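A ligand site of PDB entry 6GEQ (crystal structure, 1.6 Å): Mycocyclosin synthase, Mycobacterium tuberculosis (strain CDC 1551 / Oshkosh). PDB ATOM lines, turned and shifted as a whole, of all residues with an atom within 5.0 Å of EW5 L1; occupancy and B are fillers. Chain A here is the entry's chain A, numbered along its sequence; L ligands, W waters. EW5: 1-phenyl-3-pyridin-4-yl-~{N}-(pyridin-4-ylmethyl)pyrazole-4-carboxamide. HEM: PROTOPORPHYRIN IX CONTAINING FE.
CD2 of Leu 76 touches C07 of EW5 L1 (3.97 Å). Val 78 touches EW5 L1. Val 82 touches EW5 L1. CG2 of Val 83 touches C07 of EW5 L1, at 3.7 Å. O of Ala 167 touches C12 of EW5 L1, at 3.4 Å. Phe 168 touches EW5 L1 (CE2 to C02, 3.7 Å). O of Ala 178 touches C16 of EW5 L1, 3.9 Å away. CA of Trp 182 touches C17 of EW5 L1 (3.7 Å). Asp 185 touches EW5 L1. Val 228 touches EW5 L1. Thr 229 touches EW5 L1. Ala 233 touches EW5 L1. Hydrophobic or aromatic side chains that line EW5 L1: Leu 76, Val 78, Val 83, Ala 167, Phe 168, Trp 182, Val 228 and Ala 233. 14 residues have an atom within 4 Å of EW5 L1: Leu 76, Thr 77, Val 78, Val 82, Val 83, Ala 167, Phe 168, Ala 178, Trp 182, Asp 185, Val 228, Thr 229, Ala 233 and Gln 385.
Water W1 lies within hydrogen-bond range of N25 of EW5 L1 and ND2 of Asn 85. Water W3 lies within hydrogen-bond range of the side-chain hydroxyl of Thr 65 (2.8 Å), a nitrogen (N08) of EW5 L1 (2.9 Å) and the guanidinium group of Arg 72 (3.0 Å). Water W2 bridges the backbone NH of Thr 77 (2.9 Å) and an oxygen (O01) of EW5 L1 (3.1 Å).
An oxygen (O01) of EW5 L1 is in hydrogen-bond range of the side-chain amide nitrogen (NE2) of Gln 385, 3.1 Å away. OG1 of Thr 77 lies within hydrogen-bond range of O01 of EW5 L1 (3.2 Å).
N of Gln 385 lies within hydrogen-bond range of O of Phe 168. ND2 of Asn 85 lies within hydrogen-bond range of OG1 of Thr 229 (3.1 Å). The backbone carbonyl oxygen (O) of Ala 167 sits at hydrogen-bond distance from the side-chain hydroxyl (OG1) of Thr 77, at 2.9 Å.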
ATOM      1  N   THR A  65      -0.610   4.421  22.592  1.00  0.00           N
ATOM      2  CA  THR A  65      -1.629   3.769  21.777  1.00  0.00           C
ATOM      3  C   THR A  65      -2.582   2.909  22.615  1.00  0.00           C
ATOM      4  O   THR A  65      -3.677   2.577  22.139  1.00  0.00           O
ATOM      5  CB  THR A  65      -1.029   2.859  20.689  1.00  0.00           C
ATOM      6  OG1 THR A  65      -0.271   1.796  21.298  1.00  0.00           O
ATOM      7  CG2 THR A  65      -0.158   3.646  19.737  1.00  0.00           C
ATOM      8  N   ARG A  72      -7.848   3.444  17.470  1.00  0.00           N
ATOM      9  CA  ARG A  72      -7.132   2.174  17.452  1.00  0.00           C
ATOM     10  C   ARG A  72      -6.964   1.612  16.048  1.00  0.00           C
ATOM     11  O   ARG A  72      -7.889   1.621  15.229  1.00  0.00           O
ATOM     12  CB  ARG A  72      -7.864   1.111  18.301  1.00  0.00           C
ATOM     13  CG  ARG A  72      -8.133   1.477  19.756  1.00  0.00           C
ATOM     14  CD  ARG A  72      -8.190   0.218  20.638  1.00  0.00           C
ATOM     15  NE  ARG A  72      -6.924  -0.505  20.476  1.00  0.00           N
ATOM     16  CZ  ARG A  72      -5.801  -0.190  21.092  1.00  0.00           C
ATOM     17  NH1 ARG A  72      -4.715  -0.868  20.806  1.00  0.00           N
ATOM     18  NH2 ARG A  72      -5.788   0.787  22.002  1.00  0.00           N
ATOM     19  N   ASN A  74      -6.277  -1.673  15.814  1.00  0.00           N
ATOM     20  CA  ASN A  74      -6.885  -2.974  16.056  1.00  0.00           C
ATOM     21  C   ASN A  74      -7.037  -3.125  17.574  1.00  0.00           C
ATOM     22  O   ASN A  74      -6.564  -2.296  18.366  1.00  0.00           O
ATOM     23  CB  ASN A  74      -6.056  -4.101  15.457  1.00  0.00           C
ATOM     24  CG  ASN A  74      -4.591  -4.070  15.887  1.00  0.00           C
ATOM     25  OD1 ASN A  74      -4.245  -3.494  16.926  1.00  0.00           O
ATOM     26  ND2 ASN A  74      -3.728  -4.695  15.094  1.00  0.00           N
ATOM     27  N   LEU A  76      -6.584  -4.673  21.365  1.00  0.00           N
ATOM     28  CA  LEU A  76      -5.527  -5.269  22.150  1.00  0.00           C
ATOM     29  C   LEU A  76      -5.747  -6.767  22.309  1.00  0.00           C
ATOM     30  O   LEU A  76      -6.865  -7.225  22.575  1.00  0.00           O
ATOM     31  CB  LEU A  76      -5.468  -4.623  23.533  1.00  0.00           C
ATOM     32  CG  LEU A  76      -4.978  -3.176  23.579  1.00  0.00           C
ATOM     33  CD1 LEU A  76      -5.168  -2.634  24.981  1.00  0.00           C
ATOM     34  CD2 LEU A  76      -3.538  -3.076  23.134  1.00  0.00           C
ATOM     35  N   THR A  77      -4.672  -7.533  22.169  1.00  0.00           N
ATOM     36  CA  THR A  77      -4.678  -8.955  22.510  1.00  0.00           C
ATOM     37  C   THR A  77      -3.825  -9.236  23.744  1.00  0.00           C
ATOM     38  O   THR A  77      -3.642 -10.399  24.109  1.00  0.00           O
ATOM     39  CB  THR A  77      -4.169  -9.806  21.332  1.00  0.00           C
ATOM     40  OG1 THR A  77      -2.815  -9.460  21.036  1.00  0.00           O
ATOM     41  CG2 THR A  77      -5.041  -9.580  20.118  1.00  0.00           C
ATOM     42  N   VAL A  78      -3.330  -8.192  24.408  1.00  0.00           N
ATOM     43  CA  VAL A  78      -2.579  -8.271  25.653  1.00  0.00           C
ATOM     44  C   VAL A  78      -3.126  -7.231  26.620  1.00  0.00           C
ATOM     45  O   VAL A  78      -3.836  -6.296  26.209  1.00  0.00           O
ATOM     46  CB  VAL A  78      -1.072  -8.025  25.418  1.00  0.00           C
ATOM     47  CG1 VAL A  78      -0.464  -9.092  24.507  1.00  0.00           C
ATOM     48  CG2 VAL A  78      -0.841  -6.656  24.823  1.00  0.00           C
ATOM     49  N   VAL A  82       1.126  -4.119  28.934  1.00  0.00           N
ATOM     50  CA  VAL A  82       2.092  -4.881  28.161  1.00  0.00           C
ATOM     51  C   VAL A  82       2.447  -4.178  26.854  1.00  0.00           C
ATOM     52  O   VAL A  82       3.480  -4.477  26.253  1.00  0.00           O
ATOM     53  CB  VAL A  82       1.543  -6.297  27.928  1.00  0.00           C
ATOM     54  CG1 VAL A  82       2.491  -7.129  27.091  1.00  0.00           C
ATOM     55  CG2 VAL A  82       1.298  -6.980  29.267  1.00  0.00           C
ATOM     56  N   VAL A  83       1.634  -3.224  26.400  1.00  0.00           N
ATOM     57  CA  VAL A  83       2.048  -2.413  25.255  1.00  0.00           C
ATOM     58  C   VAL A  83       3.356  -1.696  25.538  1.00  0.00           C
ATOM     59  O   VAL A  83       4.162  -1.455  24.617  1.00  0.00           O
ATOM     60  CB  VAL A  83       0.934  -1.419  24.868  1.00  0.00           C
ATOM     61  CG1 VAL A  83       1.427  -0.485  23.760  1.00  0.00           C
ATOM     62  CG2 VAL A  83      -0.314  -2.173  24.424  1.00  0.00           C
ATOM     63  N   ASN A  85       5.849  -2.951  27.190  1.00  0.00           N
ATOM     64  CA  ASN A  85       6.632  -4.063  27.726  1.00  0.00           C
ATOM     65  C   ASN A  85       8.118  -3.711  27.846  1.00  0.00           C
ATOM     66  O   ASN A  85       8.731  -3.939  28.889  1.00  0.00           O
ATOM     67  CB  ASN A  85       6.436  -5.288  26.833  1.00  0.00           C
ATOM     68  CG  ASN A  85       7.069  -6.534  27.390  1.00  0.00           C
ATOM     69  OD1 ASN A  85       6.928  -6.861  28.570  1.00  0.00           O
ATOM     70  ND2 ASN A  85       7.787  -7.257  26.539  1.00  0.00           N
ATOM     71  N   LEU A 164      -0.392 -18.828  18.816  1.00  0.00           N
ATOM     72  CA  LEU A 164      -0.001 -17.601  18.132  1.00  0.00           C
ATOM     73  C   LEU A 164      -0.938 -17.228  16.988  1.00  0.00           C
ATOM     74  O   LEU A 164      -1.041 -16.036  16.659  1.00  0.00           O
ATOM     75  CB  LEU A 164       1.447 -17.705  17.623  1.00  0.00           C
ATOM     76  CG  LEU A 164       2.483 -17.947  18.744  1.00  0.00           C
ATOM     77  CD1 LEU A 164       3.898 -18.088  18.161  1.00  0.00           C
ATOM     78  CD2 LEU A 164       2.426 -16.851  19.812  1.00  0.00           C
ATOM     79  N   ALA A 167      -3.089 -15.119  19.133  1.00  0.00           N
ATOM     80  CA  ALA A 167      -2.380 -14.079  19.864  1.00  0.00           C
ATOM     81  C   ALA A 167      -2.015 -12.893  18.981  1.00  0.00           C
ATOM     82  O   ALA A 167      -2.035 -11.748  19.424  1.00  0.00           O
ATOM     83  CB  ALA A 167      -1.114 -14.675  20.480  1.00  0.00           C
ATOM     84  N   PHE A 168      -1.624 -13.147  17.738  1.00  0.00           N
ATOM     85  CA  PHE A 168      -1.199 -12.068  16.854  1.00  0.00           C
ATOM     86  C   PHE A 168      -2.234 -11.737  15.785  1.00  0.00           C
ATOM     87  O   PHE A 168      -1.905 -11.194  14.735  1.00  0.00           O
ATOM     88  CB  PHE A 168       0.167 -12.403  16.243  1.00  0.00           C
ATOM     89  CG  PHE A 168       1.286 -12.196  17.217  1.00  0.00           C
ATOM     90  CD1 PHE A 168       1.642 -13.193  18.104  1.00  0.00           C
ATOM     91  CD2 PHE A 168       1.928 -10.968  17.302  1.00  0.00           C
ATOM     92  CE1 PHE A 168       2.635 -12.981  19.042  1.00  0.00           C
ATOM     93  CE2 PHE A 168       2.939 -10.753  18.251  1.00  0.00           C
ATOM     94  CZ  PHE A 168       3.298 -11.766  19.113  1.00  0.00           C
ATOM     95  N   ALA A 178      -7.931 -14.896  22.849  1.00  0.00           N
ATOM     96  CA  ALA A 178      -6.614 -14.307  23.117  1.00  0.00           C
ATOM     97  C   ALA A 178      -6.358 -14.210  24.613  1.00  0.00           C
ATOM     98  O   ALA A 178      -5.231 -14.420  25.078  1.00  0.00           O
ATOM     99  CB  ALA A 178      -6.485 -12.948  22.450  1.00  0.00           C
ATOM    100  N   ASN A 181      -5.595 -17.814  25.946  1.00  0.00           N
ATOM    101  CA  ASN A 181      -4.239 -18.229  25.617  1.00  0.00           C
ATOM    102  C   ASN A 181      -3.202 -17.407  26.366  1.00  0.00           C
ATOM    103  O   ASN A 181      -2.177 -17.940  26.807  1.00  0.00           O
ATOM    104  CB  ASN A 181      -4.012 -18.128  24.101  1.00  0.00           C
ATOM    105  CG  ASN A 181      -4.782 -19.169  23.307  1.00  0.00           C
ATOM    106  OD1 ASN A 181      -5.191 -20.209  23.842  1.00  0.00           O
ATOM    107  ND2 ASN A 181      -4.958 -18.910  22.024  1.00  0.00           N
ATOM    108  N   TRP A 182      -3.434 -16.097  26.517  1.00  0.00           N
ATOM    109  CA  TRP A 182      -2.519 -15.255  27.280  1.00  0.00           C
ATOM    110  C   TRP A 182      -2.392 -15.756  28.715  1.00  0.00           C
ATOM    111  O   TRP A 182      -1.291 -15.955  29.230  1.00  0.00           O
ATOM    112  CB  TRP A 182      -2.975 -13.797  27.265  1.00  0.00           C
ATOM    113  CG  TRP A 182      -2.158 -12.908  28.177  1.00  0.00           C
ATOM    114  CD1 TRP A 182      -2.475 -12.504  29.441  1.00  0.00           C
ATOM    115  CD2 TRP A 182      -0.888 -12.313  27.876  1.00  0.00           C
ATOM    116  NE1 TRP A 182      -1.493 -11.682  29.951  1.00  0.00           N
ATOM    117  CE2 TRP A 182      -0.495 -11.560  29.012  1.00  0.00           C
ATOM    118  CE3 TRP A 182      -0.034 -12.343  26.771  1.00  0.00           C
ATOM    119  CZ2 TRP A 182       0.705 -10.854  29.059  1.00  0.00           C
ATOM    120  CZ3 TRP A 182       1.156 -11.635  26.817  1.00  0.00           C
ATOM    121  CH2 TRP A 182       1.522 -10.914  27.969  1.00  0.00           C
ATOM    122  N   ASP A 185      -0.563 -19.097  28.831  1.00  0.00           N
ATOM    123  CA  ASP A 185       0.866 -18.967  28.554  1.00  0.00           C
ATOM    124  C   ASP A 185       1.584 -18.280  29.709  1.00  0.00           C
ATOM    125  O   ASP A 185       2.747 -18.605  29.989  1.00  0.00           O
ATOM    126  CB  ASP A 185       1.075 -18.177  27.264  1.00  0.00           C
ATOM    127  CG  ASP A 185       0.655 -18.951  26.022  1.00  0.00           C
ATOM    128  OD1 ASP A 185       0.331 -20.159  26.138  1.00  0.00           O
ATOM    129  OD2 ASP A 185       0.653 -18.354  24.913  1.00  0.00           O
ATOM    130  N   VAL A 228       6.508 -14.814  27.780  1.00  0.00           N
ATOM    131  CA  VAL A 228       5.416 -14.947  26.822  1.00  0.00           C
ATOM    132  C   VAL A 228       5.655 -14.023  25.630  1.00  0.00           C
ATOM    133  O   VAL A 228       5.539 -14.436  24.465  1.00  0.00           O
ATOM    134  CB  VAL A 228       4.058 -14.655  27.482  1.00  0.00           C
ATOM    135  CG1 VAL A 228       2.930 -14.738  26.457  1.00  0.00           C
ATOM    136  CG2 VAL A 228       3.792 -15.620  28.615  1.00  0.00           C
ATOM    137  N   THR A 229       5.988 -12.764  25.905  1.00  0.00           N
ATOM    138  CA  THR A 229       6.105 -11.782  24.831  1.00  0.00           C
ATOM    139  C   THR A 229       7.304 -12.069  23.944  1.00  0.00           C
ATOM    140  O   THR A 229       7.246 -11.843  22.726  1.00  0.00           O
ATOM    141  CB  THR A 229       6.209 -10.368  25.392  1.00  0.00           C
ATOM    142  OG1 THR A 229       7.318 -10.264  26.287  1.00  0.00           O
ATOM    143  CG2 THR A 229       4.935  -9.979  26.106  1.00  0.00           C
ATOM    144  N   ALA A 233       6.626 -13.007  20.088  1.00  0.00           N
ATOM    145  CA  ALA A 233       7.113 -12.089  19.072  1.00  0.00           C
ATOM    146  C   ALA A 233       8.215 -12.727  18.236  1.00  0.00           C
ATOM    147  O   ALA A 233       8.229 -12.605  17.005  1.00  0.00           O
ATOM    148  CB  ALA A 233       7.598 -10.792  19.723  1.00  0.00           C
ATOM    149  N   PRO A 285       1.908   1.275  14.687  1.00  0.00           N
ATOM    150  CA  PRO A 285       1.077   2.356  15.267  1.00  0.00           C
ATOM    151  C   PRO A 285       1.779   3.205  16.311  1.00  0.00           C
ATOM    152  O   PRO A 285       2.593   2.720  17.103  1.00  0.00           O
ATOM    153  CB  PRO A 285      -0.098   1.595  15.898  1.00  0.00           C
ATOM    154  CG  PRO A 285       0.487   0.249  16.289  1.00  0.00           C
ATOM    155  CD  PRO A 285       1.602  -0.045  15.282  1.00  0.00           C
ATOM    156  N   GLN A 385      -1.612  -9.934  12.210  1.00  0.00           N
ATOM    157  CA  GLN A 385      -0.561  -8.924  12.261  1.00  0.00           C
ATOM    158  C   GLN A 385       0.608  -9.251  11.337  1.00  0.00           C
ATOM    159  O   GLN A 385       1.477  -8.389  11.135  1.00  0.00           O
ATOM    160  CB  GLN A 385      -0.074  -8.741  13.701  1.00  0.00           C
ATOM    161  CG  GLN A 385      -1.124  -8.172  14.618  1.00  0.00           C
ATOM    162  CD  GLN A 385      -0.634  -7.996  16.027  1.00  0.00           C
ATOM    163  OE1 GLN A 385       0.476  -7.516  16.238  1.00  0.00           O
ATOM    164  NE2 GLN A 385      -1.461  -8.366  17.001  1.00  0.00           N
HETATM  165  C10 EW5 L   1       0.804  -3.946  18.608  1.00  0.00           C
HETATM  166  C15 EW5 L   1      -1.051 -12.548  23.206  1.00  0.00           C
HETATM  167  C17 EW5 L   1      -0.854 -14.841  23.995  1.00  0.00           C
HETATM  168  C21 EW5 L   1       2.392  -9.672  22.178  1.00  0.00           C
HETATM  169  C22 EW5 L   1       3.554  -8.867  22.420  1.00  0.00           C
HETATM  170  C24 EW5 L   1       5.957  -8.437  22.382  1.00  0.00           C
HETATM  171  C26 EW5 L   1       4.572  -6.857  23.364  1.00  0.00           C
HETATM  172  C02 EW5 L   1       1.006  -8.390  20.284  1.00  0.00           C
HETATM  173  C04 EW5 L   1       1.725  -6.326  18.913  1.00  0.00           C
HETATM  174  C05 EW5 L   1       1.007  -5.065  19.416  1.00  0.00           C
HETATM  175  C06 EW5 L   1       0.494  -4.995  20.725  1.00  0.00           C
HETATM  176  C07 EW5 L   1      -0.165  -3.826  21.172  1.00  0.00           C
HETATM  177  C09 EW5 L   1       0.123  -2.811  19.109  1.00  0.00           C
HETATM  178  C11 EW5 L   1       1.240  -9.466  21.256  1.00  0.00           C
HETATM  179  C12 EW5 L   1       0.393 -10.544  21.497  1.00  0.00           C
HETATM  180  C14 EW5 L   1       0.346 -12.528  22.993  1.00  0.00           C
HETATM  181  C16 EW5 L   1      -1.651 -13.698  23.709  1.00  0.00           C
HETATM  182  C18 EW5 L   1       0.525 -14.805  23.782  1.00  0.00           C
HETATM  183  C19 EW5 L   1       1.133 -13.651  23.289  1.00  0.00           C
HETATM  184  C23 EW5 L   1       4.853  -9.267  22.077  1.00  0.00           C
HETATM  185  C27 EW5 L   1       3.427  -7.634  23.095  1.00  0.00           C
HETATM  186  N03 EW5 L   1       1.957  -7.410  19.890  1.00  0.00           N
HETATM  187  N08 EW5 L   1      -0.353  -2.740  20.373  1.00  0.00           N
HETATM  188  N13 EW5 L   1       0.935 -11.371  22.496  1.00  0.00           N
HETATM  189  N20 EW5 L   1       2.147 -10.829  22.890  1.00  0.00           N
HETATM  190  N25 EW5 L   1       5.822  -7.233  23.026  1.00  0.00           N
HETATM  191  O01 EW5 L   1      -0.128  -8.318  19.762  1.00  0.00           O
HETATM  192  CHA HEM L   2      10.013  -5.006  17.793  1.00  0.00           C
HETATM  193  CHB HEM L   2      10.356  -6.947  13.373  1.00  0.00           C
HETATM  194  CHC HEM L   2      12.413 -10.888  15.331  1.00  0.00           C
HETATM  195  CHD HEM L   2      11.068  -9.344  19.697  1.00  0.00           C
HETATM  196  C1A HEM L   2      10.000  -5.138  16.420  1.00  0.00           C
HETATM  197  C2A HEM L   2       9.637  -4.108  15.465  1.00  0.00           C
HETATM  198  C3A HEM L   2       9.736  -4.668  14.243  1.00  0.00           C
HETATM  199  C4A HEM L   2      10.152  -6.040  14.390  1.00  0.00           C
HETATM  200  CMA HEM L   2       9.467  -3.978  12.880  1.00  0.00           C
HETATM  201  CAA HEM L   2       9.262  -2.637  15.801  1.00  0.00           C
HETATM  202  CBA HEM L   2       7.817  -2.483  16.256  1.00  0.00           C
HETATM  203  CGA HEM L   2       7.473  -1.031  16.511  1.00  0.00           C
HETATM  204  O1A HEM L   2       8.389  -0.160  16.542  1.00  0.00           O
HETATM  205  O2A HEM L   2       6.258  -0.728  16.697  1.00  0.00           O
HETATM  206  C1B HEM L   2      10.972  -8.177  13.509  1.00  0.00           C
HETATM  207  C2B HEM L   2      11.382  -9.046  12.428  1.00  0.00           C
HETATM  208  C3B HEM L   2      11.950 -10.148  12.987  1.00  0.00           C
HETATM  209  C4B HEM L   2      11.906  -9.997  14.413  1.00  0.00           C
HETATM  210  CMB HEM L   2      11.180  -8.752  10.935  1.00  0.00           C
HETATM  211  CAB HEM L   2      12.574 -11.386  12.309  1.00  0.00           C
HETATM  212  CBB HEM L   2      13.047 -11.380  11.057  1.00  0.00           C
HETATM  213  C1C HEM L   2      12.270 -10.806  16.687  1.00  0.00           C
HETATM  214  C2C HEM L   2      12.793 -11.750  17.661  1.00  0.00           C
HETATM  215  C3C HEM L   2      12.413 -11.318  18.891  1.00  0.00           C
HETATM  216  C4C HEM L   2      11.651 -10.101  18.704  1.00  0.00           C
HETATM  217  CMC HEM L   2      13.617 -12.998  17.276  1.00  0.00           C
HETATM  218  CAC HEM L   2      12.668 -11.919  20.281  1.00  0.00           C
HETATM  219  CBC HEM L   2      13.333 -13.069  20.490  1.00  0.00           C
HETATM  220  C1D HEM L   2      10.634  -8.056  19.541  1.00  0.00           C
HETATM  221  C2D HEM L   2      10.142  -7.219  20.600  1.00  0.00           C
HETATM  222  C3D HEM L   2       9.835  -6.001  20.087  1.00  0.00           C
HETATM  223  C4D HEM L   2      10.153  -6.045  18.676  1.00  0.00           C
HETATM  224  CMD HEM L   2       9.965  -7.682  22.058  1.00  0.00           C
HETATM  225  CAD HEM L   2       9.267  -4.787  20.842  1.00  0.00           C
HETATM  226  CBD HEM L   2      10.382  -3.773  21.083  1.00  0.00           C
HETATM  227  CGD HEM L   2       9.910  -2.512  21.771  1.00  0.00           C
HETATM  228  O1D HEM L   2      10.765  -1.648  22.070  1.00  0.00           O
HETATM  229  O2D HEM L   2       8.697  -2.362  22.037  1.00  0.00           O
HETATM  230  NA  HEM L   2      10.297  -6.314  15.737  1.00  0.00           N
HETATM  231  NB  HEM L   2      11.295  -8.790  14.701  1.00  0.00           N
HETATM  232  NC  HEM L   2      11.589  -9.805  17.362  1.00  0.00           N
HETATM  233  ND  HEM L   2      10.637  -7.305  18.375  1.00  0.00           N
HETATM  234 FE   HEM L   2      11.097  -8.011  16.544  1.00  0.00          FE
HETATM  235  O   HOH W   1       7.935  -5.508  23.917  1.00  0.00           O
HETATM  236  O   HOH W   2      -2.202  -6.543  21.143  1.00  0.00           O
HETATM  237  O   HOH W   3      -1.848  -0.525  21.479  1.00  0.00           O
HETATM  238  O   HOH W   4       3.570 -16.298  23.049  1.00  0.00           O
